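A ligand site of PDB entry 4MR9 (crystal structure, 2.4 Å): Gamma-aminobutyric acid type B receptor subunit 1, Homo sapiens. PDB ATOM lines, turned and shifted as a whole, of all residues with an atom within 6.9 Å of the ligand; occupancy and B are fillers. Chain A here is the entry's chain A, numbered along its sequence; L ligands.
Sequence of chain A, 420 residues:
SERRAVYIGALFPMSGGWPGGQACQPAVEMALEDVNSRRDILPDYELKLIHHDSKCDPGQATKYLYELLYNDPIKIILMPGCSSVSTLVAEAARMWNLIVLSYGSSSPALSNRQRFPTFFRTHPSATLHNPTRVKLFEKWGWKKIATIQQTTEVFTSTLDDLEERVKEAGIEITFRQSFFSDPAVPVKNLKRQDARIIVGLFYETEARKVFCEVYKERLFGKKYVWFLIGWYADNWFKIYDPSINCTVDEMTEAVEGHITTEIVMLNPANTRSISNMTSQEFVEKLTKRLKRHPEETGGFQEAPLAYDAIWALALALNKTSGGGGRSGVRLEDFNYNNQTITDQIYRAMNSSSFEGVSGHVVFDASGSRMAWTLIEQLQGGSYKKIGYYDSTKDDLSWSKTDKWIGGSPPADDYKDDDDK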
ATOM      1  N   TRP A  18      17.273 -22.209  19.414  1.00  0.00           N
ATOM      2  CA  TRP A  18      17.948 -21.431  20.458  1.00  0.00           C
ATOM      3  C   TRP A  18      18.199 -22.396  21.620  1.00  0.00           C
ATOM      4  O   TRP A  18      17.287 -22.606  22.413  1.00  0.00           O
ATOM      5  CB  TRP A  18      17.180 -20.185  20.881  1.00  0.00           C
ATOM      6  CG  TRP A  18      17.818 -19.422  22.006  1.00  0.00           C
ATOM      7  CD1 TRP A  18      18.910 -18.608  21.929  1.00  0.00           C
ATOM      8  CD2 TRP A  18      17.381 -19.380  23.389  1.00  0.00           C
ATOM      9  NE1 TRP A  18      19.215 -18.112  23.173  1.00  0.00           N
ATOM     10  CE2 TRP A  18      18.266 -18.542  24.074  1.00  0.00           C
ATOM     11  CE3 TRP A  18      16.317 -19.969  24.096  1.00  0.00           C
ATOM     12  CZ2 TRP A  18      18.144 -18.277  25.444  1.00  0.00           C
ATOM     13  CZ3 TRP A  18      16.190 -19.723  25.452  1.00  0.00           C
ATOM     14  CH2 TRP A  18      17.091 -18.867  26.120  1.00  0.00           C
ATOM     15  N   CYS A  56      13.620 -26.942  22.137  1.00  0.00           N
ATOM     16  CA  CYS A  56      13.179 -25.707  21.461  1.00  0.00           C
ATOM     17  C   CYS A  56      12.064 -26.095  20.463  1.00  0.00           C
ATOM     18  O   CYS A  56      11.887 -25.500  19.393  1.00  0.00           O
ATOM     19  CB  CYS A  56      14.366 -25.032  20.794  1.00  0.00           C
ATOM     20  SG  CYS A  56      14.192 -23.257  20.496  1.00  0.00           S
ATOM     21  N   GLY A  81      11.441 -21.485  27.885  1.00  0.00           N
ATOM     22  CA  GLY A  81      12.512 -20.676  27.320  1.00  0.00           C
ATOM     23  C   GLY A  81      12.253 -20.095  25.937  1.00  0.00           C
ATOM     24  O   GLY A  81      12.158 -18.871  25.802  1.00  0.00           O
ATOM     25  N   CYS A  82      12.143 -20.984  24.885  1.00  0.00           N
ATOM     26  CA  CYS A  82      11.908 -20.619  23.471  1.00  0.00           C
ATOM     27  C   CYS A  82      10.542 -19.956  23.277  1.00  0.00           C
ATOM     28  O   CYS A  82       9.574 -20.357  23.919  1.00  0.00           O
ATOM     29  CB  CYS A  82      12.101 -21.806  22.514  1.00  0.00           C
ATOM     30  SG  CYS A  82      13.854 -22.252  22.274  1.00  0.00           S
ATOM     31  N   SER A  83      10.467 -18.988  22.378  1.00  0.00           N
ATOM     32  CA  SER A  83       9.242 -18.280  21.946  1.00  0.00           C
ATOM     33  C   SER A  83       8.147 -19.218  21.471  1.00  0.00           C
ATOM     34  O   SER A  83       7.015 -19.019  21.861  1.00  0.00           O
ATOM     35  CB  SER A  83       9.563 -17.290  20.837  1.00  0.00           C
ATOM     36  OG  SER A  83       9.951 -16.044  21.378  1.00  0.00           O
ATOM     37  N   SER A  84       8.489 -20.259  20.662  1.00  0.00           N
ATOM     38  CA  SER A  84       7.519 -21.243  20.167  1.00  0.00           C
ATOM     39  C   SER A  84       6.993 -22.114  21.298  1.00  0.00           C
ATOM     40  O   SER A  84       5.825 -22.512  21.263  1.00  0.00           O
ATOM     41  CB  SER A  84       8.103 -22.107  19.060  1.00  0.00           C
ATOM     42  OG  SER A  84       9.173 -22.893  19.577  1.00  0.00           O
ATOM     43  N   VAL A  85       7.845 -22.439  22.286  1.00  0.00           N
ATOM     44  CA  VAL A  85       7.419 -23.257  23.426  1.00  0.00           C
ATOM     45  C   VAL A  85       6.511 -22.385  24.349  1.00  0.00           C
ATOM     46  O   VAL A  85       5.438 -22.822  24.764  1.00  0.00           O
ATOM     47  CB  VAL A  85       8.631 -23.910  24.140  1.00  0.00           C
ATOM     48  CG1 VAL A  85       8.232 -24.586  25.461  1.00  0.00           C
ATOM     49  CG2 VAL A  85       9.345 -24.915  23.212  1.00  0.00           C
ATOM     50  N   TYR A 103      12.119 -16.906  30.471  1.00  0.00           N
ATOM     51  CA  TYR A 103      13.430 -16.295  30.656  1.00  0.00           C
ATOM     52  C   TYR A 103      14.101 -16.042  29.285  1.00  0.00           C
ATOM     53  O   TYR A 103      15.112 -15.355  29.224  1.00  0.00           O
ATOM     54  CB  TYR A 103      14.298 -17.215  31.589  1.00  0.00           C
ATOM     55  CG  TYR A 103      14.391 -18.649  31.089  1.00  0.00           C
ATOM     56  CD1 TYR A 103      15.335 -19.013  30.134  1.00  0.00           C
ATOM     57  CD2 TYR A 103      13.456 -19.590  31.476  1.00  0.00           C
ATOM     58  CE1 TYR A 103      15.334 -20.285  29.571  1.00  0.00           C
ATOM     59  CE2 TYR A 103      13.451 -20.883  30.944  1.00  0.00           C
ATOM     60  CZ  TYR A 103      14.399 -21.223  29.989  1.00  0.00           C
ATOM     61  OH  TYR A 103      14.400 -22.458  29.431  1.00  0.00           O
ATOM     62  N   GLY A 104      13.538 -16.574  28.194  1.00  0.00           N
ATOM     63  CA  GLY A 104      14.175 -16.387  26.894  1.00  0.00           C
ATOM     64  C   GLY A 104      13.350 -16.009  25.674  1.00  0.00           C
ATOM     65  O   GLY A 104      13.902 -15.890  24.606  1.00  0.00           O
ATOM     66  N   SER A 105      12.040 -15.804  25.798  1.00  0.00           N
ATOM     67  CA  SER A 105      11.185 -15.509  24.636  1.00  0.00           C
ATOM     68  C   SER A 105      11.181 -14.043  24.200  1.00  0.00           C
ATOM     69  O   SER A 105      10.792 -13.184  24.966  1.00  0.00           O
ATOM     70  CB  SER A 105       9.772 -15.993  24.901  1.00  0.00           C
ATOM     71  OG  SER A 105       9.798 -17.346  25.275  1.00  0.00           O
ATOM     72  N   SER A 106      11.602 -13.778  22.961  1.00  0.00           N
ATOM     73  CA  SER A 106      11.665 -12.413  22.403  1.00  0.00           C
ATOM     74  C   SER A 106      10.481 -12.076  21.450  1.00  0.00           C
ATOM     75  O   SER A 106      10.372 -10.928  21.028  1.00  0.00           O
ATOM     76  CB  SER A 106      12.972 -12.214  21.637  1.00  0.00           C
ATOM     77  OG  SER A 106      12.972 -13.050  20.496  1.00  0.00           O
ATOM     78  N   SER A 107       9.637 -13.068  21.106  1.00  0.00           N
ATOM     79  CA  SER A 107       8.511 -12.921  20.202  1.00  0.00           C
ATOM     80  C   SER A 107       7.546 -11.793  20.580  1.00  0.00           C
ATOM     81  O   SER A 107       6.899 -11.863  21.614  1.00  0.00           O
ATOM     82  CB  SER A 107       7.752 -14.241  20.053  1.00  0.00           C
ATOM     83  OG  SER A 107       6.596 -14.177  19.252  1.00  0.00           O
ATOM     84  N   ARG A 121       7.725 -12.222  31.266  1.00  0.00           N
ATOM     85  CA  ARG A 121       9.016 -12.566  30.684  1.00  0.00           C
ATOM     86  C   ARG A 121      10.104 -11.601  31.101  1.00  0.00           C
ATOM     87  O   ARG A 121       9.915 -10.410  30.971  1.00  0.00           O
ATOM     88  CB  ARG A 121       8.934 -12.723  29.152  1.00  0.00           C
ATOM     89  CG  ARG A 121       8.386 -11.517  28.378  1.00  0.00           C
ATOM     90  CD  ARG A 121       8.539 -11.786  26.913  1.00  0.00           C
ATOM     91  NE  ARG A 121       7.690 -10.938  26.082  1.00  0.00           N
ATOM     92  CZ  ARG A 121       7.587 -11.049  24.771  1.00  0.00           C
ATOM     93  NH1 ARG A 121       8.255 -11.988  24.117  1.00  0.00           N
ATOM     94  NH2 ARG A 121       6.779 -10.239  24.095  1.00  0.00           N
ATOM     95  N   HIS A 123      12.899 -11.626  29.709  1.00  0.00           N
ATOM     96  CA  HIS A 123      13.445 -11.365  28.419  1.00  0.00           C
ATOM     97  C   HIS A 123      12.530 -10.338  27.753  1.00  0.00           C
ATOM     98  O   HIS A 123      11.303 -10.546  27.668  1.00  0.00           O
ATOM     99  CB  HIS A 123      13.503 -12.630  27.561  1.00  0.00           C
ATOM    100  CG  HIS A 123      14.320 -12.463  26.334  1.00  0.00           C
ATOM    101  ND1 HIS A 123      14.071 -11.542  25.337  1.00  0.00           N
ATOM    102  CD2 HIS A 123      15.461 -13.223  25.983  1.00  0.00           C
ATOM    103  CE1 HIS A 123      15.039 -11.717  24.475  1.00  0.00           C
ATOM    104  NE2 HIS A 123      15.879 -12.663  24.741  1.00  0.00           N
ATOM    105  N   PRO A 124      13.059  -9.220  27.261  1.00  0.00           N
ATOM    106  CA  PRO A 124      12.189  -8.250  26.571  1.00  0.00           C
ATOM    107  C   PRO A 124      11.741  -8.748  25.212  1.00  0.00           C
ATOM    108  O   PRO A 124      12.326  -9.686  24.604  1.00  0.00           O
ATOM    109  CB  PRO A 124      13.130  -7.044  26.395  1.00  0.00           C
ATOM    110  CG  PRO A 124      14.267  -7.276  27.305  1.00  0.00           C
ATOM    111  CD  PRO A 124      14.456  -8.750  27.278  1.00  0.00           C
ATOM    112  N   HIS A 129      13.619  -2.881  20.535  1.00  0.00           N
ATOM    113  CA  HIS A 129      14.602  -2.263  19.628  1.00  0.00           C
ATOM    114  C   HIS A 129      14.048  -0.988  18.975  1.00  0.00           C
ATOM    115  O   HIS A 129      14.820  -0.093  18.647  1.00  0.00           O
ATOM    116  CB  HIS A 129      15.000  -3.243  18.520  1.00  0.00           C
ATOM    117  CG  HIS A 129      15.816  -4.415  18.966  1.00  0.00           C
ATOM    118  ND1 HIS A 129      17.144  -4.533  18.637  1.00  0.00           N
ATOM    119  CD2 HIS A 129      15.437  -5.508  19.662  1.00  0.00           C
ATOM    120  CE1 HIS A 129      17.534  -5.690  19.150  1.00  0.00           C
ATOM    121  NE2 HIS A 129      16.539  -6.311  19.780  1.00  0.00           N
ATOM    122  N   VAL A 154       8.330 -12.958  13.709  1.00  0.00           N
ATOM    123  CA  VAL A 154       9.038 -12.030  14.599  1.00  0.00           C
ATOM    124  C   VAL A 154       9.412 -10.713  13.920  1.00  0.00           C
ATOM    125  O   VAL A 154       9.211  -9.668  14.522  1.00  0.00           O
ATOM    126  CB  VAL A 154      10.234 -12.660  15.345  1.00  0.00           C
ATOM    127  CG1 VAL A 154       9.740 -13.619  16.421  1.00  0.00           C
ATOM    128  CG2 VAL A 154      11.220 -13.355  14.393  1.00  0.00           C
ATOM    129  N   TYR A 203      17.692 -12.935   9.961  1.00  0.00           N
ATOM    130  CA  TYR A 203      18.654 -13.740  10.707  1.00  0.00           C
ATOM    131  C   TYR A 203      20.043 -13.660  10.051  1.00  0.00           C
ATOM    132  O   TYR A 203      20.169 -13.204   8.912  1.00  0.00           O
ATOM    133  CB  TYR A 203      18.181 -15.206  10.857  1.00  0.00           C
ATOM    134  CG  TYR A 203      17.022 -15.334  11.828  1.00  0.00           C
ATOM    135  CD1 TYR A 203      17.175 -15.013  13.169  1.00  0.00           C
ATOM    136  CD2 TYR A 203      15.760 -15.738  11.386  1.00  0.00           C
ATOM    137  CE1 TYR A 203      16.093 -15.079  14.065  1.00  0.00           C
ATOM    138  CE2 TYR A 203      14.684 -15.830  12.272  1.00  0.00           C
ATOM    139  CZ  TYR A 203      14.858 -15.508  13.604  1.00  0.00           C
ATOM    140  OH  TYR A 203      13.794 -15.606  14.450  1.00  0.00           O
ATOM    141  N   TRP A 231      22.558  -9.008  17.804  1.00  0.00           N
ATOM    142  CA  TRP A 231      22.914 -10.318  18.373  1.00  0.00           C
ATOM    143  C   TRP A 231      23.547 -11.329  17.450  1.00  0.00           C
ATOM    144  O   TRP A 231      23.677 -12.481  17.854  1.00  0.00           O
ATOM    145  CB  TRP A 231      21.840 -10.904  19.299  1.00  0.00           C
ATOM    146  CG  TRP A 231      20.436 -10.871  18.750  1.00  0.00           C
ATOM    147  CD1 TRP A 231      19.410 -10.074  19.163  1.00  0.00           C
ATOM    148  CD2 TRP A 231      19.906 -11.691  17.708  1.00  0.00           C
ATOM    149  NE1 TRP A 231      18.282 -10.318  18.419  1.00  0.00           N
ATOM    150  CE2 TRP A 231      18.553 -11.325  17.531  1.00  0.00           C
ATOM    151  CE3 TRP A 231      20.443 -12.725  16.907  1.00  0.00           C
ATOM    152  CZ2 TRP A 231      17.724 -11.941  16.594  1.00  0.00           C
ATOM    153  CZ3 TRP A 231      19.626 -13.310  15.934  1.00  0.00           C
ATOM    154  CH2 TRP A 231      18.282 -12.896  15.780  1.00  0.00           C
ATOM    155  N   ILE A 263      19.478  -5.781  23.253  1.00  0.00           N
ATOM    156  CA  ILE A 263      19.065  -5.710  24.659  1.00  0.00           C
ATOM    157  C   ILE A 263      20.263  -5.978  25.582  1.00  0.00           C
ATOM    158  O   ILE A 263      21.083  -6.854  25.303  1.00  0.00           O
ATOM    159  CB  ILE A 263      17.878  -6.677  24.918  1.00  0.00           C
ATOM    160  CG1 ILE A 263      16.611  -6.131  24.247  1.00  0.00           C
ATOM    161  CG2 ILE A 263      17.659  -6.919  26.423  1.00  0.00           C
ATOM    162  CD1 ILE A 263      15.814  -7.150  23.521  1.00  0.00           C
ATOM    163  N   MET A 265      21.667  -7.500  28.614  1.00  0.00           N
ATOM    164  CA  MET A 265      21.338  -8.662  29.447  1.00  0.00           C
ATOM    165  C   MET A 265      22.124  -8.806  30.743  1.00  0.00           C
ATOM    166  O   MET A 265      21.734  -9.564  31.615  1.00  0.00           O
ATOM    167  CB  MET A 265      21.347  -9.935  28.620  1.00  0.00           C
ATOM    168  CG  MET A 265      20.171  -9.999  27.709  1.00  0.00           C
ATOM    169  SD  MET A 265      20.288 -11.335  26.558  1.00  0.00           S
ATOM    170  CE  MET A 265      18.890 -10.973  25.558  1.00  0.00           C
ATOM    171  N   GLN A 301      24.471 -15.524  27.227  1.00  0.00           N
ATOM    172  CA  GLN A 301      24.100 -14.102  27.336  1.00  0.00           C
ATOM    173  C   GLN A 301      22.772 -13.895  28.010  1.00  0.00           C
ATOM    174  O   GLN A 301      22.629 -12.949  28.775  1.00  0.00           O
ATOM    175  CB  GLN A 301      24.148 -13.426  25.965  1.00  0.00           C
ATOM    176  CG  GLN A 301      25.596 -13.165  25.508  1.00  0.00           C
ATOM    177  CD  GLN A 301      25.699 -12.421  24.200  1.00  0.00           C
ATOM    178  OE1 GLN A 301      24.785 -12.415  23.364  1.00  0.00           O
ATOM    179  NE2 GLN A 301      26.848 -11.792  23.971  1.00  0.00           N
ATOM    180  N   GLU A 302      21.795 -14.807  27.758  1.00  0.00           N
ATOM    181  CA  GLU A 302      20.459 -14.775  28.358  1.00  0.00           C
ATOM    182  C   GLU A 302      20.421 -15.283  29.785  1.00  0.00           C
ATOM    183  O   GLU A 302      19.463 -14.991  30.484  1.00  0.00           O
ATOM    184  CB  GLU A 302      19.475 -15.589  27.517  1.00  0.00           C
ATOM    185  CG  GLU A 302      19.104 -14.929  26.217  1.00  0.00           C
ATOM    186  CD  GLU A 302      20.090 -15.140  25.085  1.00  0.00           C
ATOM    187  OE1 GLU A 302      20.874 -16.114  25.115  1.00  0.00           O
ATOM    188  OE2 GLU A 302      20.036 -14.337  24.143  1.00  0.00           O
ATOM    189  N   LEU A 305      18.876 -13.316  32.778  1.00  0.00           N
ATOM    190  CA  LEU A 305      17.424 -13.167  32.701  1.00  0.00           C
ATOM    191  C   LEU A 305      16.775 -14.378  33.366  1.00  0.00           C
ATOM    192  O   LEU A 305      15.748 -14.218  34.019  1.00  0.00           O
ATOM    193  CB  LEU A 305      16.930 -13.042  31.236  1.00  0.00           C
ATOM    194  CG  LEU A 305      17.705 -12.092  30.297  1.00  0.00           C
ATOM    195  CD1 LEU A 305      17.255 -12.262  28.885  1.00  0.00           C
ATOM    196  CD2 LEU A 305      17.551 -10.663  30.703  1.00  0.00           C
HETATM  197  O1  LIG L   1      12.909 -15.872  21.230  1.00  0.00           O
HETATM  198  C1  LIG L   1      13.566 -16.913  21.421  1.00  0.00           C
HETATM  199  O2  LIG L   1      12.904 -18.048  21.296  1.00  0.00           O
HETATM  200  C2  LIG L   1      15.028 -16.933  21.782  1.00  0.00           C
HETATM  201  C3  LIG L   1      15.568 -15.522  22.020  1.00  0.00           C
HETATM  202  C4  LIG L   1      16.780 -15.560  22.960  1.00  0.00           C
HETATM  203  N1  LIG L   1      17.596 -14.348  22.789  1.00  0.00           N
HETATM  204  C5  LIG L   1      17.767 -13.666  21.506  1.00  0.00           C
HETATM  205  C6  LIG L   1      18.242 -12.240  21.786  1.00  0.00           C
HETATM  206  C7  LIG L   1      18.791 -14.390  20.616  1.00  0.00           C
HETATM  207  C8  LIG L   1      16.417 -13.611  20.765  1.00  0.00           C
HETATM  208  O3  LIG L   1      15.834 -14.930  20.734  1.00  0.00           O
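OG of Ser 106 is in hydrogen-bond range of O1 of the ligand (2.9 Å). The backbone NH of Ser 83 lies within hydrogen-bond range of an oxygen (O2) of the ligand. N1 of the ligand lies within salt-bridge range of OE2 of Glu 302, 2.8 Å away. The side-chain hydroxyl of Ser 83 sits at hydrogen-bond distance from an oxygen (O1) of the ligand (3.0 Å). A nitrogen (N1) of the ligand lies within hydrogen-bond range of a ring nitrogen (NE2) of His 123, at 3.1 Å. N of Ser 106 sits at hydrogen-bond distance from O1 of the ligand (3.0 Å).
The side-chain sulfur (SG) of Cys 56 forms a disulfide with the side-chain sulfur (SG) of Cys 82, at 2.1 Å. The backbone NH (N) of Ser 83 is in hydrogen-bond range of the side-chain hydroxyl (OG) of Ser 105 (3.4 Å). The side-chain hydroxyl (OG) of Ser 83 sits at hydrogen-bond distance from the backbone NH (N) of Ser 107. The backbone NH (N) of Trp 18 sits at hydrogen-bond distance from the side-chain sulfur (SG) of Cys 56, 3.4 Å away. The side-chain hydroxyl (OG) of Ser 83 sits at hydrogen-bond distance from the backbone NH (N) of Ser 106 (3.2 Å). O of Cys 82 sits at hydrogen-bond distance from OG of Ser 105 (3.3 Å). OE1 of Glu 302 sits at hydrogen-bond distance from NE1 of Trp 18 (3.2 Å). O of Ser 105 sits at hydrogen-bond distance from NH1 of Arg 121.
Residues that only touch the ligand: Gly 104 (3.1 Å), Cys 82 (3.5 Å), Trp 18 (3.5 Å), Trp 231 (3.6 Å) and Ser 105 (3.8 Å). Hydrophobic or aromatic side chains that line the ligand: Trp 18 and Trp 231. Of the 24 residues printed, 9 come within 4 Å of the ligand. The nearest printed residue that does not touch the ligand is Met 265 (4.03 Å).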
